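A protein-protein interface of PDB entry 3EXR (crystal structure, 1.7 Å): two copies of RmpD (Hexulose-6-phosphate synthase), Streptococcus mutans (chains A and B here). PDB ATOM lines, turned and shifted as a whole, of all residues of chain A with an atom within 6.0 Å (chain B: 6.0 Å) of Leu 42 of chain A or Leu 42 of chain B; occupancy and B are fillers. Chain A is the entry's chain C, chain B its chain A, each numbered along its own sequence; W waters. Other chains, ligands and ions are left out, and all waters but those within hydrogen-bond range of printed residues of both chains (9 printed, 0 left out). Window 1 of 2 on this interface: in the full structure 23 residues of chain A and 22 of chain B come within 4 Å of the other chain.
Water W3 lies within hydrogen-bond range of the side-chain amide oxygen of Gln 43 of chain A (2.7 Å), the side-chain amide nitrogen of Asn 78 of chain B (3.1 Å) and the backbone carbonyl oxygen of Leu 42 of chain A (3.3 Å).
Water W2 lies within hydrogen-bond range of O of Gln 43 of chain A (2.7 Å) and OG of Ser 46 of chain B (3.4 Å).
Water W1 lies within hydrogen-bond range of the backbone carbonyl oxygen (O) of Gln 43 of chain B (2.8 Å) and the side-chain hydroxyl (OG) of Ser 46 of chain A (3.3 Å).
Water W4 bridges O of Leu 42 of chain A (2.8 Å) and OD1 of Asn 78 of chain B (2.9 Å).
Water W6 lies within hydrogen-bond range of the backbone carbonyl oxygen (O) of Val 44 of chain B (2.9 Å), the backbone NH (N) of Glu 47 of chain B (3.1 Å), the backbone carbonyl oxygen (O) of Gln 43 of chain A (3.3 Å) and the backbone NH (N) of Ser 46 of chain B (3.4 Å).
Water W8 lies within hydrogen-bond range of O of Thr 65 of chain B (3.1 Å) and O of Thr 65 of chain A (3.2 Å).
The backbone carbonyl oxygen of Val 74 of chain A lies within hydrogen-bond range of the side-chain amide nitrogen of Asn 78 of chain A (2.9 Å).
O of Val 74 of chain B sits at hydrogen-bond distance from ND2 of Asn 78 of chain B, at 2.9 Å.
The side-chain hydroxyl (OG1) of Thr 65 of chain A lies close to the backbone NH (N) of Cys 67 of chain A, at 3.5 Å.
The side-chain hydroxyl (OG1) of Thr 65 of chain B lies close to the backbone NH (N) of Cys 67 of chain B (3.4 Å).
Gly 37 of chain A touches none of the printed residues of chain B.
Printed residues of chain B within 4 Å of Val 39 of chain A: Val 74 (3.7 Å).
Printed residues of chain B within 4 Å of Gln 43 of chain A: Gly 45 (3.3 Å) and Ser 46 (2.7 Å).
Of the printed residues of chain B, Thr 65 of chain A touches Leu 42.
Leu 42 of chain B touches four residues of chain A.
Of the printed residues of chain A, Ser 46 of chain B touches Leu 42 and Gln 43.
Printed residues of chain A within 4 Å of Thr 65 of chain B: Leu 42 (3.9 Å).
The nearest printed residue of chain B that does not touch Leu 42 of chain A is Val 74 of chain B (4.01 Å).
The nearest residue of chain A that does not touch Leu 42 of chain B is Val 74 of chain A (4.1 Å).
The nearest printed residue of chain B that does not touch Leu 41 of chain A is Leu 42 of chain B (4.1 Å).
CG2 of Val 74 of chain B touches CG2 of Val 39 of chain A, at 3.7 Å.
Leu 41 of chain A touches Leu 41 of chain B.
CD2 of Leu 42 of chain A touches CD2 of Leu 42 of chain B, at 3.8 Å.
Gln 43 of chain A touches Gly 45 of chain B (O to CA, 3.3 Å).
Val 44 of chain A touches Gly 45 of chain B (N to CA, 3.9 Å).
Gly 45 of chain A touches Leu 42 of chain B.
Gln 43 of chain B touches Gly 45 of chain A (O to CA, 3.3 Å).
Gly 45 of chain A touches Val 44 of chain B (CA to N, 3.9 Å).
Leu 42 of chain B touches Thr 65 of chain A.
Val 39 of chain B touches Val 74 of chain A (CG2 to CG2, 3.9 Å).
Of the 16 printed residues of chain B, 9 touch a printed residue of chain A.
Of the 16 printed residues of chain A, 9 touch a printed residue of chain B.
Among the printed residues, 17 pairs touch across the chains.
Among the printed residues, no Asp or Glu carboxylate lies within 4 Å of a Lys or Arg side-chain nitrogen of the other chain.
Leu 42 of chain B touches its own counterpart, Leu 42 of chain A.
Leu 42 of chain A touches Gly 45 of chain B, and with the chains exchanged Gly 45 of chain A touches Leu 42 of chain B.
Gln 43 of chain A touches Gly 45 of chain B, and with the chains exchanged Gly 45 of chain A touches Gln 43 of chain B.
Gly 45 of chain B touches its own counterpart, Gly 45 of chain A.
Positions printed for both chains: 37, 38, 39, 40, 41, 42, 43, 44, 45, 46, 47, 64, 65, 67, 74 and 78.
Of the 17 pairs that touch across the chains among the printed residues, 17 have their exchanged pair printed and touching as well.
The side-chain hydroxyl of Ser 46 of chain A lies within hydrogen-bond range of the side-chain amide oxygen of Gln 43 of chain B (2.8 Å).
N of Ser 46 of chain B is in hydrogen-bond range of O of Leu 42 of chain A (3.3 Å).
OG of Ser 46 of chain B is in hydrogen-bond range of OE1 of Gln 43 of chain A (2.7 Å).
The backbone NH (N) of Ser 46 of chain A is in hydrogen-bond range of the backbone carbonyl oxygen (O) of Leu 42 of chain B (3.2 Å).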
ATOM      1  N   GLY A  37     -15.076  15.860 -12.599  1.00  0.00           N
ATOM      2  CA  GLY A  37     -15.032  14.522 -12.026  1.00  0.00           C
ATOM      3  C   GLY A  37     -13.638  14.034 -11.709  1.00  0.00           C
ATOM      4  O   GLY A  37     -12.620  14.531 -12.246  1.00  0.00           O
ATOM      5  N   THR A  38     -13.584  13.057 -10.802  1.00  0.00           N
ATOM      6  CA  THR A  38     -12.312  12.515 -10.359  1.00  0.00           C
ATOM      7  C   THR A  38     -11.427  12.008 -11.507  1.00  0.00           C
ATOM      8  O   THR A  38     -10.225  12.265 -11.529  1.00  0.00           O
ATOM      9  CB  THR A  38     -12.493  11.377  -9.318  1.00  0.00           C
ATOM     10  OG1 THR A  38     -13.584  11.663  -8.444  1.00  0.00           O
ATOM     11  CG2 THR A  38     -11.243  11.259  -8.472  1.00  0.00           C
ATOM     12  N   VAL A  39     -12.022  11.288 -12.445  1.00  0.00           N
ATOM     13  CA  VAL A  39     -11.272  10.731 -13.568  1.00  0.00           C
ATOM     14  C   VAL A  39     -10.575  11.854 -14.319  1.00  0.00           C
ATOM     15  O   VAL A  39      -9.434  11.718 -14.730  1.00  0.00           O
ATOM     16  CB  VAL A  39     -12.197   9.920 -14.548  1.00  0.00           C
ATOM     17  CG1 VAL A  39     -11.481   9.610 -15.845  1.00  0.00           C
ATOM     18  CG2 VAL A  39     -12.717   8.634 -13.894  1.00  0.00           C
ATOM     19  N   CYS A  40     -11.281  12.968 -14.488  1.00  0.00           N
ATOM     20  CA  CYS A  40     -10.724  14.095 -15.200  1.00  0.00           C
ATOM     21  C   CYS A  40      -9.657  14.827 -14.388  1.00  0.00           C
ATOM     22  O   CYS A  40      -8.576  15.113 -14.903  1.00  0.00           O
ATOM     23  CB  CYS A  40     -11.846  15.047 -15.615  1.00  0.00           C
ATOM     24  SG  CYS A  40     -11.308  16.178 -16.866  1.00  0.00           S
ATOM     25  N   LEU A  41      -9.948  15.146 -13.130  1.00  0.00           N
ATOM     26  CA  LEU A  41      -8.949  15.837 -12.309  1.00  0.00           C
ATOM     27  C   LEU A  41      -7.660  15.019 -12.198  1.00  0.00           C
ATOM     28  O   LEU A  41      -6.581  15.592 -12.249  1.00  0.00           O
ATOM     29  CB  LEU A  41      -9.507  16.125 -10.908  1.00  0.00           C
ATOM     30  CG  LEU A  41     -10.622  17.171 -10.804  1.00  0.00           C
ATOM     31  CD1 LEU A  41     -11.231  17.129  -9.428  1.00  0.00           C
ATOM     32  CD2 LEU A  41     -10.068  18.532 -11.159  1.00  0.00           C
ATOM     33  N   LEU A  42      -7.745  13.693 -12.070  1.00  0.00           N
ATOM     34  CA  LEU A  42      -6.511  12.868 -12.016  1.00  0.00           C
ATOM     35  C   LEU A  42      -5.687  12.893 -13.306  1.00  0.00           C
ATOM     36  O   LEU A  42      -4.472  12.659 -13.299  1.00  0.00           O
ATOM     37  CB  LEU A  42      -6.830  11.419 -11.615  1.00  0.00           C
ATOM     38  CG  LEU A  42      -7.315  11.216 -10.176  1.00  0.00           C
ATOM     39  CD1 LEU A  42      -7.947   9.871 -10.028  1.00  0.00           C
ATOM     40  CD2 LEU A  42      -6.165  11.367  -9.184  1.00  0.00           C
ATOM     41  N   GLN A  43      -6.347  13.192 -14.418  1.00  0.00           N
ATOM     42  CA  GLN A  43      -5.674  13.370 -15.697  1.00  0.00           C
ATOM     43  C   GLN A  43      -5.079  14.744 -15.923  1.00  0.00           C
ATOM     44  O   GLN A  43      -3.984  14.864 -16.489  1.00  0.00           O
ATOM     45  CB  GLN A  43      -6.651  13.090 -16.835  1.00  0.00           C
ATOM     46  CG  GLN A  43      -6.863  11.582 -17.094  1.00  0.00           C
ATOM     47  CD  GLN A  43      -5.603  10.897 -17.636  1.00  0.00           C
ATOM     48  OE1 GLN A  43      -4.717  10.533 -16.867  1.00  0.00           O
ATOM     49  NE2 GLN A  43      -5.530  10.730 -18.951  1.00  0.00           N
ATOM     50  N   VAL A  44      -5.846  15.783 -15.584  1.00  0.00           N
ATOM     51  CA  VAL A  44      -5.524  17.129 -16.049  1.00  0.00           C
ATOM     52  C   VAL A  44      -5.146  18.102 -14.929  1.00  0.00           C
ATOM     53  O   VAL A  44      -4.681  19.202 -15.196  1.00  0.00           O
ATOM     54  CB  VAL A  44      -6.699  17.741 -16.889  1.00  0.00           C
ATOM     55  CG1 VAL A  44      -7.138  16.796 -18.018  1.00  0.00           C
ATOM     56  CG2 VAL A  44      -7.862  18.140 -16.001  1.00  0.00           C
ATOM     57  N   GLY A  45      -5.376  17.708 -13.678  1.00  0.00           N
ATOM     58  CA  GLY A  45      -5.090  18.578 -12.561  1.00  0.00           C
ATOM     59  C   GLY A  45      -6.164  19.635 -12.339  1.00  0.00           C
ATOM     60  O   GLY A  45      -7.237  19.640 -12.985  1.00  0.00           O
ATOM     61  N   SER A  46      -5.891  20.544 -11.413  1.00  0.00           N
ATOM     62  CA  SER A  46      -6.941  21.420 -10.885  1.00  0.00           C
ATOM     63  C   SER A  46      -7.183  22.682 -11.711  1.00  0.00           C
ATOM     64  O   SER A  46      -8.142  23.436 -11.438  1.00  0.00           O
ATOM     65  CB  SER A  46      -6.623  21.800  -9.460  1.00  0.00           C
ATOM     66  OG  SER A  46      -5.492  22.642  -9.423  1.00  0.00           O
ATOM     67  N   GLU A  47      -6.327  22.974 -12.688  1.00  0.00           N
ATOM     68  CA  GLU A  47      -6.626  24.164 -13.535  1.00  0.00           C
ATOM     69  C   GLU A  47      -8.023  24.104 -14.148  1.00  0.00           C
ATOM     70  O   GLU A  47      -8.657  25.139 -14.323  1.00  0.00           O
ATOM     71  CB  GLU A  47      -5.579  24.420 -14.609  1.00  0.00           C
ATOM     72  CG  GLU A  47      -5.719  25.791 -15.240  1.00  0.00           C
ATOM     73  CD  GLU A  47      -4.578  26.151 -16.144  1.00  0.00           C
ATOM     74  OE1 GLU A  47      -3.881  25.234 -16.642  1.00  0.00           O
ATOM     75  OE2 GLU A  47      -4.397  27.362 -16.346  1.00  0.00           O
ATOM     76  N   ASP A  64     -14.463  17.186  -7.711  1.00  0.00           N
ATOM     77  CA  ASP A  64     -14.734  15.809  -7.260  1.00  0.00           C
ATOM     78  C   ASP A  64     -13.414  15.085  -6.984  1.00  0.00           C
ATOM     79  O   ASP A  64     -12.988  14.234  -7.756  1.00  0.00           O
ATOM     80  CB  ASP A  64     -15.606  15.116  -8.309  1.00  0.00           C
ATOM     81  CG  ASP A  64     -15.965  13.697  -7.973  1.00  0.00           C
ATOM     82  OD1 ASP A  64     -15.963  13.305  -6.764  1.00  0.00           O
ATOM     83  OD2 ASP A  64     -16.270  12.937  -8.931  1.00  0.00           O
ATOM     84  N   THR A  65     -12.751  15.434  -5.886  1.00  0.00           N
ATOM     85  CA  THR A  65     -11.451  14.841  -5.594  1.00  0.00           C
ATOM     86  C   THR A  65     -11.545  13.529  -4.830  1.00  0.00           C
ATOM     87  O   THR A  65     -10.538  12.828  -4.701  1.00  0.00           O
ATOM     88  CB  THR A  65     -10.610  15.810  -4.773  1.00  0.00           C
ATOM     89  OG1 THR A  65     -11.323  16.104  -3.559  1.00  0.00           O
ATOM     90  CG2 THR A  65     -10.387  17.129  -5.532  1.00  0.00           C
ATOM     91  N   CYS A  67     -11.447  13.104  -1.809  1.00  0.00           N
ATOM     92  CA  CYS A  67     -10.353  13.260  -0.890  1.00  0.00           C
ATOM     93  C   CYS A  67     -10.440  12.238   0.242  1.00  0.00           C
ATOM     94  O   CYS A  67     -11.478  12.125   0.897  1.00  0.00           O
ATOM     95  CB  CYS A  67     -10.396  14.674  -0.338  1.00  0.00           C
ATOM     96  SG  CYS A  67      -9.175  15.047   0.905  1.00  0.00           S
ATOM     97  N   VAL A  74      -5.866  19.521   0.178  1.00  0.00           N
ATOM     98  CA  VAL A  74      -6.669  19.274  -1.016  1.00  0.00           C
ATOM     99  C   VAL A  74      -7.791  20.300  -1.175  1.00  0.00           C
ATOM    100  O   VAL A  74      -8.005  20.839  -2.269  1.00  0.00           O
ATOM    101  CB  VAL A  74      -7.156  17.810  -1.104  1.00  0.00           C
ATOM    102  CG1 VAL A  74      -7.961  17.586  -2.354  1.00  0.00           C
ATOM    103  CG2 VAL A  74      -5.982  16.858  -1.116  1.00  0.00           C
ATOM    104  N   ASN A  78      -8.179  23.244  -4.327  1.00  0.00           N
ATOM    105  CA  ASN A  78      -9.356  23.357  -5.184  1.00  0.00           C
ATOM    106  C   ASN A  78     -10.182  24.592  -4.920  1.00  0.00           C
ATOM    107  O   ASN A  78     -10.778  25.159  -5.861  1.00  0.00           O
ATOM    108  CB  ASN A  78     -10.154  22.070  -5.113  1.00  0.00           C
ATOM    109  CG  ASN A  78      -9.430  20.951  -5.814  1.00  0.00           C
ATOM    110  OD1 ASN A  78      -9.484  20.852  -7.030  1.00  0.00           O
ATOM    111  ND2 ASN A  78      -8.668  20.162  -5.056  1.00  0.00           N
ATOM    112  N   GLY B  37       2.135  11.230  -5.446  1.00  0.00           N
ATOM    113  CA  GLY B  37       1.098  11.197  -4.435  1.00  0.00           C
ATOM    114  C   GLY B  37      -0.214  11.823  -4.877  1.00  0.00           C
ATOM    115  O   GLY B  37      -0.243  12.637  -5.798  1.00  0.00           O
ATOM    116  N   THR B  38      -1.312  11.473  -4.197  1.00  0.00           N
ATOM    117  CA  THR B  38      -2.652  11.914  -4.608  1.00  0.00           C
ATOM    118  C   THR B  38      -2.763  13.435  -4.624  1.00  0.00           C
ATOM    119  O   THR B  38      -3.351  14.007  -5.542  1.00  0.00           O
ATOM    120  CB  THR B  38      -3.731  11.385  -3.654  1.00  0.00           C
ATOM    121  OG1 THR B  38      -3.465  10.015  -3.320  1.00  0.00           O
ATOM    122  CG2 THR B  38      -5.091  11.460  -4.307  1.00  0.00           C
ATOM    123  N   VAL B  39      -2.214  14.099  -3.602  1.00  0.00           N
ATOM    124  CA  VAL B  39      -2.278  15.564  -3.557  1.00  0.00           C
ATOM    125  C   VAL B  39      -1.667  16.171  -4.832  1.00  0.00           C
ATOM    126  O   VAL B  39      -2.149  17.167  -5.371  1.00  0.00           O
ATOM    127  CB  VAL B  39      -1.529  16.110  -2.310  1.00  0.00           C
ATOM    128  CG1 VAL B  39      -1.378  17.624  -2.422  1.00  0.00           C
ATOM    129  CG2 VAL B  39      -2.260  15.699  -1.026  1.00  0.00           C
ATOM    130  N   CYS B  40      -0.571  15.582  -5.281  1.00  0.00           N
ATOM    131  CA  CYS B  40       0.146  16.061  -6.446  1.00  0.00           C
ATOM    132  C   CYS B  40      -0.613  15.746  -7.734  1.00  0.00           C
ATOM    133  O   CYS B  40      -0.787  16.621  -8.579  1.00  0.00           O
ATOM    134  CB  CYS B  40       1.552  15.464  -6.505  1.00  0.00           C
ATOM    135  SG  CYS B  40       2.611  16.420  -7.599  1.00  0.00           S
ATOM    136  N   LEU B  41      -1.063  14.501  -7.882  1.00  0.00           N
ATOM    137  CA  LEU B  41      -1.824  14.140  -9.065  1.00  0.00           C
ATOM    138  C   LEU B  41      -3.094  14.977  -9.233  1.00  0.00           C
ATOM    139  O   LEU B  41      -3.429  15.395 -10.346  1.00  0.00           O
ATOM    140  CB  LEU B  41      -2.150  12.651  -9.077  1.00  0.00           C
ATOM    141  CG  LEU B  41      -0.943  11.715  -9.252  1.00  0.00           C
ATOM    142  CD1 LEU B  41      -1.421  10.313  -9.068  1.00  0.00           C
ATOM    143  CD2 LEU B  41      -0.328  11.901 -10.651  1.00  0.00           C
ATOM    144  N   LEU B  42      -3.819  15.230  -8.147  1.00  0.00           N
ATOM    145  CA  LEU B  42      -5.012  16.083  -8.261  1.00  0.00           C
ATOM    146  C   LEU B  42      -4.677  17.495  -8.664  1.00  0.00           C
ATOM    147  O   LEU B  42      -5.542  18.184  -9.213  1.00  0.00           O
ATOM    148  CB  LEU B  42      -5.829  16.085  -6.954  1.00  0.00           C
ATOM    149  CG  LEU B  42      -6.475  14.751  -6.576  1.00  0.00           C
ATOM    150  CD1 LEU B  42      -6.913  14.775  -5.127  1.00  0.00           C
ATOM    151  CD2 LEU B  42      -7.616  14.430  -7.514  1.00  0.00           C
ATOM    152  N   GLN B  43      -3.457  17.952  -8.356  1.00  0.00           N
ATOM    153  CA  GLN B  43      -2.997  19.271  -8.801  1.00  0.00           C
ATOM    154  C   GLN B  43      -2.486  19.322 -10.236  1.00  0.00           C
ATOM    155  O   GLN B  43      -2.770  20.270 -10.944  1.00  0.00           O
ATOM    156  CB  GLN B  43      -1.897  19.811  -7.883  1.00  0.00           C
ATOM    157  CG  GLN B  43      -2.370  20.385  -6.594  1.00  0.00           C
ATOM    158  CD  GLN B  43      -3.175  21.651  -6.774  1.00  0.00           C
ATOM    159  OE1 GLN B  43      -4.363  21.601  -7.069  1.00  0.00           O
ATOM    160  NE2 GLN B  43      -2.531  22.794  -6.561  1.00  0.00           N
ATOM    161  N   VAL B  44      -1.712  18.316 -10.655  1.00  0.00           N
ATOM    162  CA  VAL B  44      -0.953  18.426 -11.899  1.00  0.00           C
ATOM    163  C   VAL B  44      -1.355  17.446 -12.979  1.00  0.00           C
ATOM    164  O   VAL B  44      -0.968  17.639 -14.121  1.00  0.00           O
ATOM    165  CB  VAL B  44       0.549  18.367 -11.672  1.00  0.00           C
ATOM    166  CG1 VAL B  44       0.944  19.318 -10.543  1.00  0.00           C
ATOM    167  CG2 VAL B  44       0.985  16.960 -11.367  1.00  0.00           C
ATOM    168  N   GLY B  45      -2.119  16.419 -12.632  1.00  0.00           N
ATOM    169  CA  GLY B  45      -2.566  15.412 -13.592  1.00  0.00           C
ATOM    170  C   GLY B  45      -1.485  14.368 -13.813  1.00  0.00           C
ATOM    171  O   GLY B  45      -0.456  14.373 -13.128  1.00  0.00           O
ATOM    172  N   SER B  46      -1.700  13.524 -14.811  1.00  0.00           N
ATOM    173  CA  SER B  46      -0.951  12.284 -14.952  1.00  0.00           C
ATOM    174  C   SER B  46       0.330  12.440 -15.747  1.00  0.00           C
ATOM    175  O   SER B  46       1.129  11.511 -15.804  1.00  0.00           O
ATOM    176  CB  SER B  46      -1.846  11.209 -15.557  1.00  0.00           C
ATOM    177  OG  SER B  46      -2.239  11.547 -16.883  1.00  0.00           O
ATOM    178  N   GLU B  47       0.558  13.589 -16.362  1.00  0.00           N
ATOM    179  CA  GLU B  47       1.782  13.759 -17.133  1.00  0.00           C
ATOM    180  C   GLU B  47       3.018  13.573 -16.214  1.00  0.00           C
ATOM    181  O   GLU B  47       4.042  13.072 -16.635  1.00  0.00           O
ATOM    182  CB  GLU B  47       1.823  15.060 -17.931  1.00  0.00           C
ATOM    183  CG  GLU B  47       3.059  15.163 -18.822  1.00  0.00           C
ATOM    184  CD  GLU B  47       3.075  16.351 -19.767  1.00  0.00           C
ATOM    185  OE1 GLU B  47       2.477  17.405 -19.465  1.00  0.00           O
ATOM    186  OE2 GLU B  47       3.757  16.229 -20.807  1.00  0.00           O
ATOM    187  N   ASP B  64      -0.515   7.240  -7.225  1.00  0.00           N
ATOM    188  CA  ASP B  64      -1.314   7.159  -6.002  1.00  0.00           C
ATOM    189  C   ASP B  64      -2.644   7.865  -6.237  1.00  0.00           C
ATOM    190  O   ASP B  64      -2.868   8.943  -5.728  1.00  0.00           O
ATOM    191  CB  ASP B  64      -0.513   7.767  -4.856  1.00  0.00           C
ATOM    192  CG  ASP B  64      -1.231   7.764  -3.528  1.00  0.00           C
ATOM    193  OD1 ASP B  64      -2.153   6.972  -3.284  1.00  0.00           O
ATOM    194  OD2 ASP B  64      -0.865   8.588  -2.657  1.00  0.00           O
ATOM    195  N   THR B  65      -3.529   7.226  -6.999  1.00  0.00           N
ATOM    196  CA  THR B  65      -4.816   7.847  -7.320  1.00  0.00           C
ATOM    197  C   THR B  65      -5.898   7.610  -6.264  1.00  0.00           C
ATOM    198  O   THR B  65      -6.930   8.269  -6.280  1.00  0.00           O
ATOM    199  CB  THR B  65      -5.384   7.322  -8.643  1.00  0.00           C
ATOM    200  OG1 THR B  65      -5.539   5.905  -8.558  1.00  0.00           O
ATOM    201  CG2 THR B  65      -4.433   7.574  -9.777  1.00  0.00           C
ATOM    202  N   CYS B  67      -7.981   5.433  -6.189  1.00  0.00           N
ATOM    203  CA  CYS B  67      -9.140   5.209  -7.053  1.00  0.00           C
ATOM    204  C   CYS B  67     -10.308   4.541  -6.337  1.00  0.00           C
ATOM    205  O   CYS B  67     -10.144   3.507  -5.680  1.00  0.00           O
ATOM    206  CB  CYS B  67      -8.705   4.390  -8.257  1.00  0.00           C
ATOM    207  SG  CYS B  67     -10.017   3.868  -9.301  1.00  0.00           S
ATOM    208  N   VAL B  74      -9.202   4.703 -14.852  1.00  0.00           N
ATOM    209  CA  VAL B  74      -8.141   5.396 -14.098  1.00  0.00           C
ATOM    210  C   VAL B  74      -6.820   4.573 -14.183  1.00  0.00           C
ATOM    211  O   VAL B  74      -5.725   5.135 -14.371  1.00  0.00           O
ATOM    212  CB  VAL B  74      -8.599   5.693 -12.633  1.00  0.00           C
ATOM    213  CG1 VAL B  74      -7.441   6.295 -11.774  1.00  0.00           C
ATOM    214  CG2 VAL B  74      -9.885   6.562 -12.595  1.00  0.00           C
ATOM    215  N   ASN B  78      -3.269   5.840 -16.101  1.00  0.00           N
ATOM    216  CA  ASN B  78      -1.960   5.938 -15.467  1.00  0.00           C
ATOM    217  C   ASN B  78      -0.972   4.900 -15.961  1.00  0.00           C
ATOM    218  O   ASN B  78       0.208   5.192 -15.980  1.00  0.00           O
ATOM    219  CB  ASN B  78      -2.094   5.899 -13.950  1.00  0.00           C
ATOM    220  CG  ASN B  78      -2.686   7.170 -13.412  1.00  0.00           C
ATOM    221  OD1 ASN B  78      -1.980   8.153 -13.223  1.00  0.00           O
ATOM    222  ND2 ASN B  78      -4.000   7.173 -13.222  1.00  0.00           N
HETATM  223  O   HOH W   1      -2.307  22.946 -10.341  1.00  0.00           O
HETATM  224  O   HOH W   2      -3.446  13.903 -18.984  1.00  0.00           O
HETATM  225  O   HOH W   3      -5.338   9.686 -14.379  1.00  0.00           O
HETATM  226  O   HOH W   4      -3.616  10.247 -12.172  1.00  0.00           O
HETATM  227  O   HOH W   5      -8.024  18.583  -7.891  1.00  0.00           O
HETATM  228  O   HOH W   6      -1.026  16.251 -16.664  1.00  0.00           O
HETATM  229  O   HOH W   7      -5.998  19.536  -6.154  1.00  0.00           O
HETATM  230  O   HOH W   8      -8.386  10.992  -6.102  1.00  0.00           O
HETATM  231  O   HOH W   9      -3.862  21.606 -13.816  1.00  0.00           O
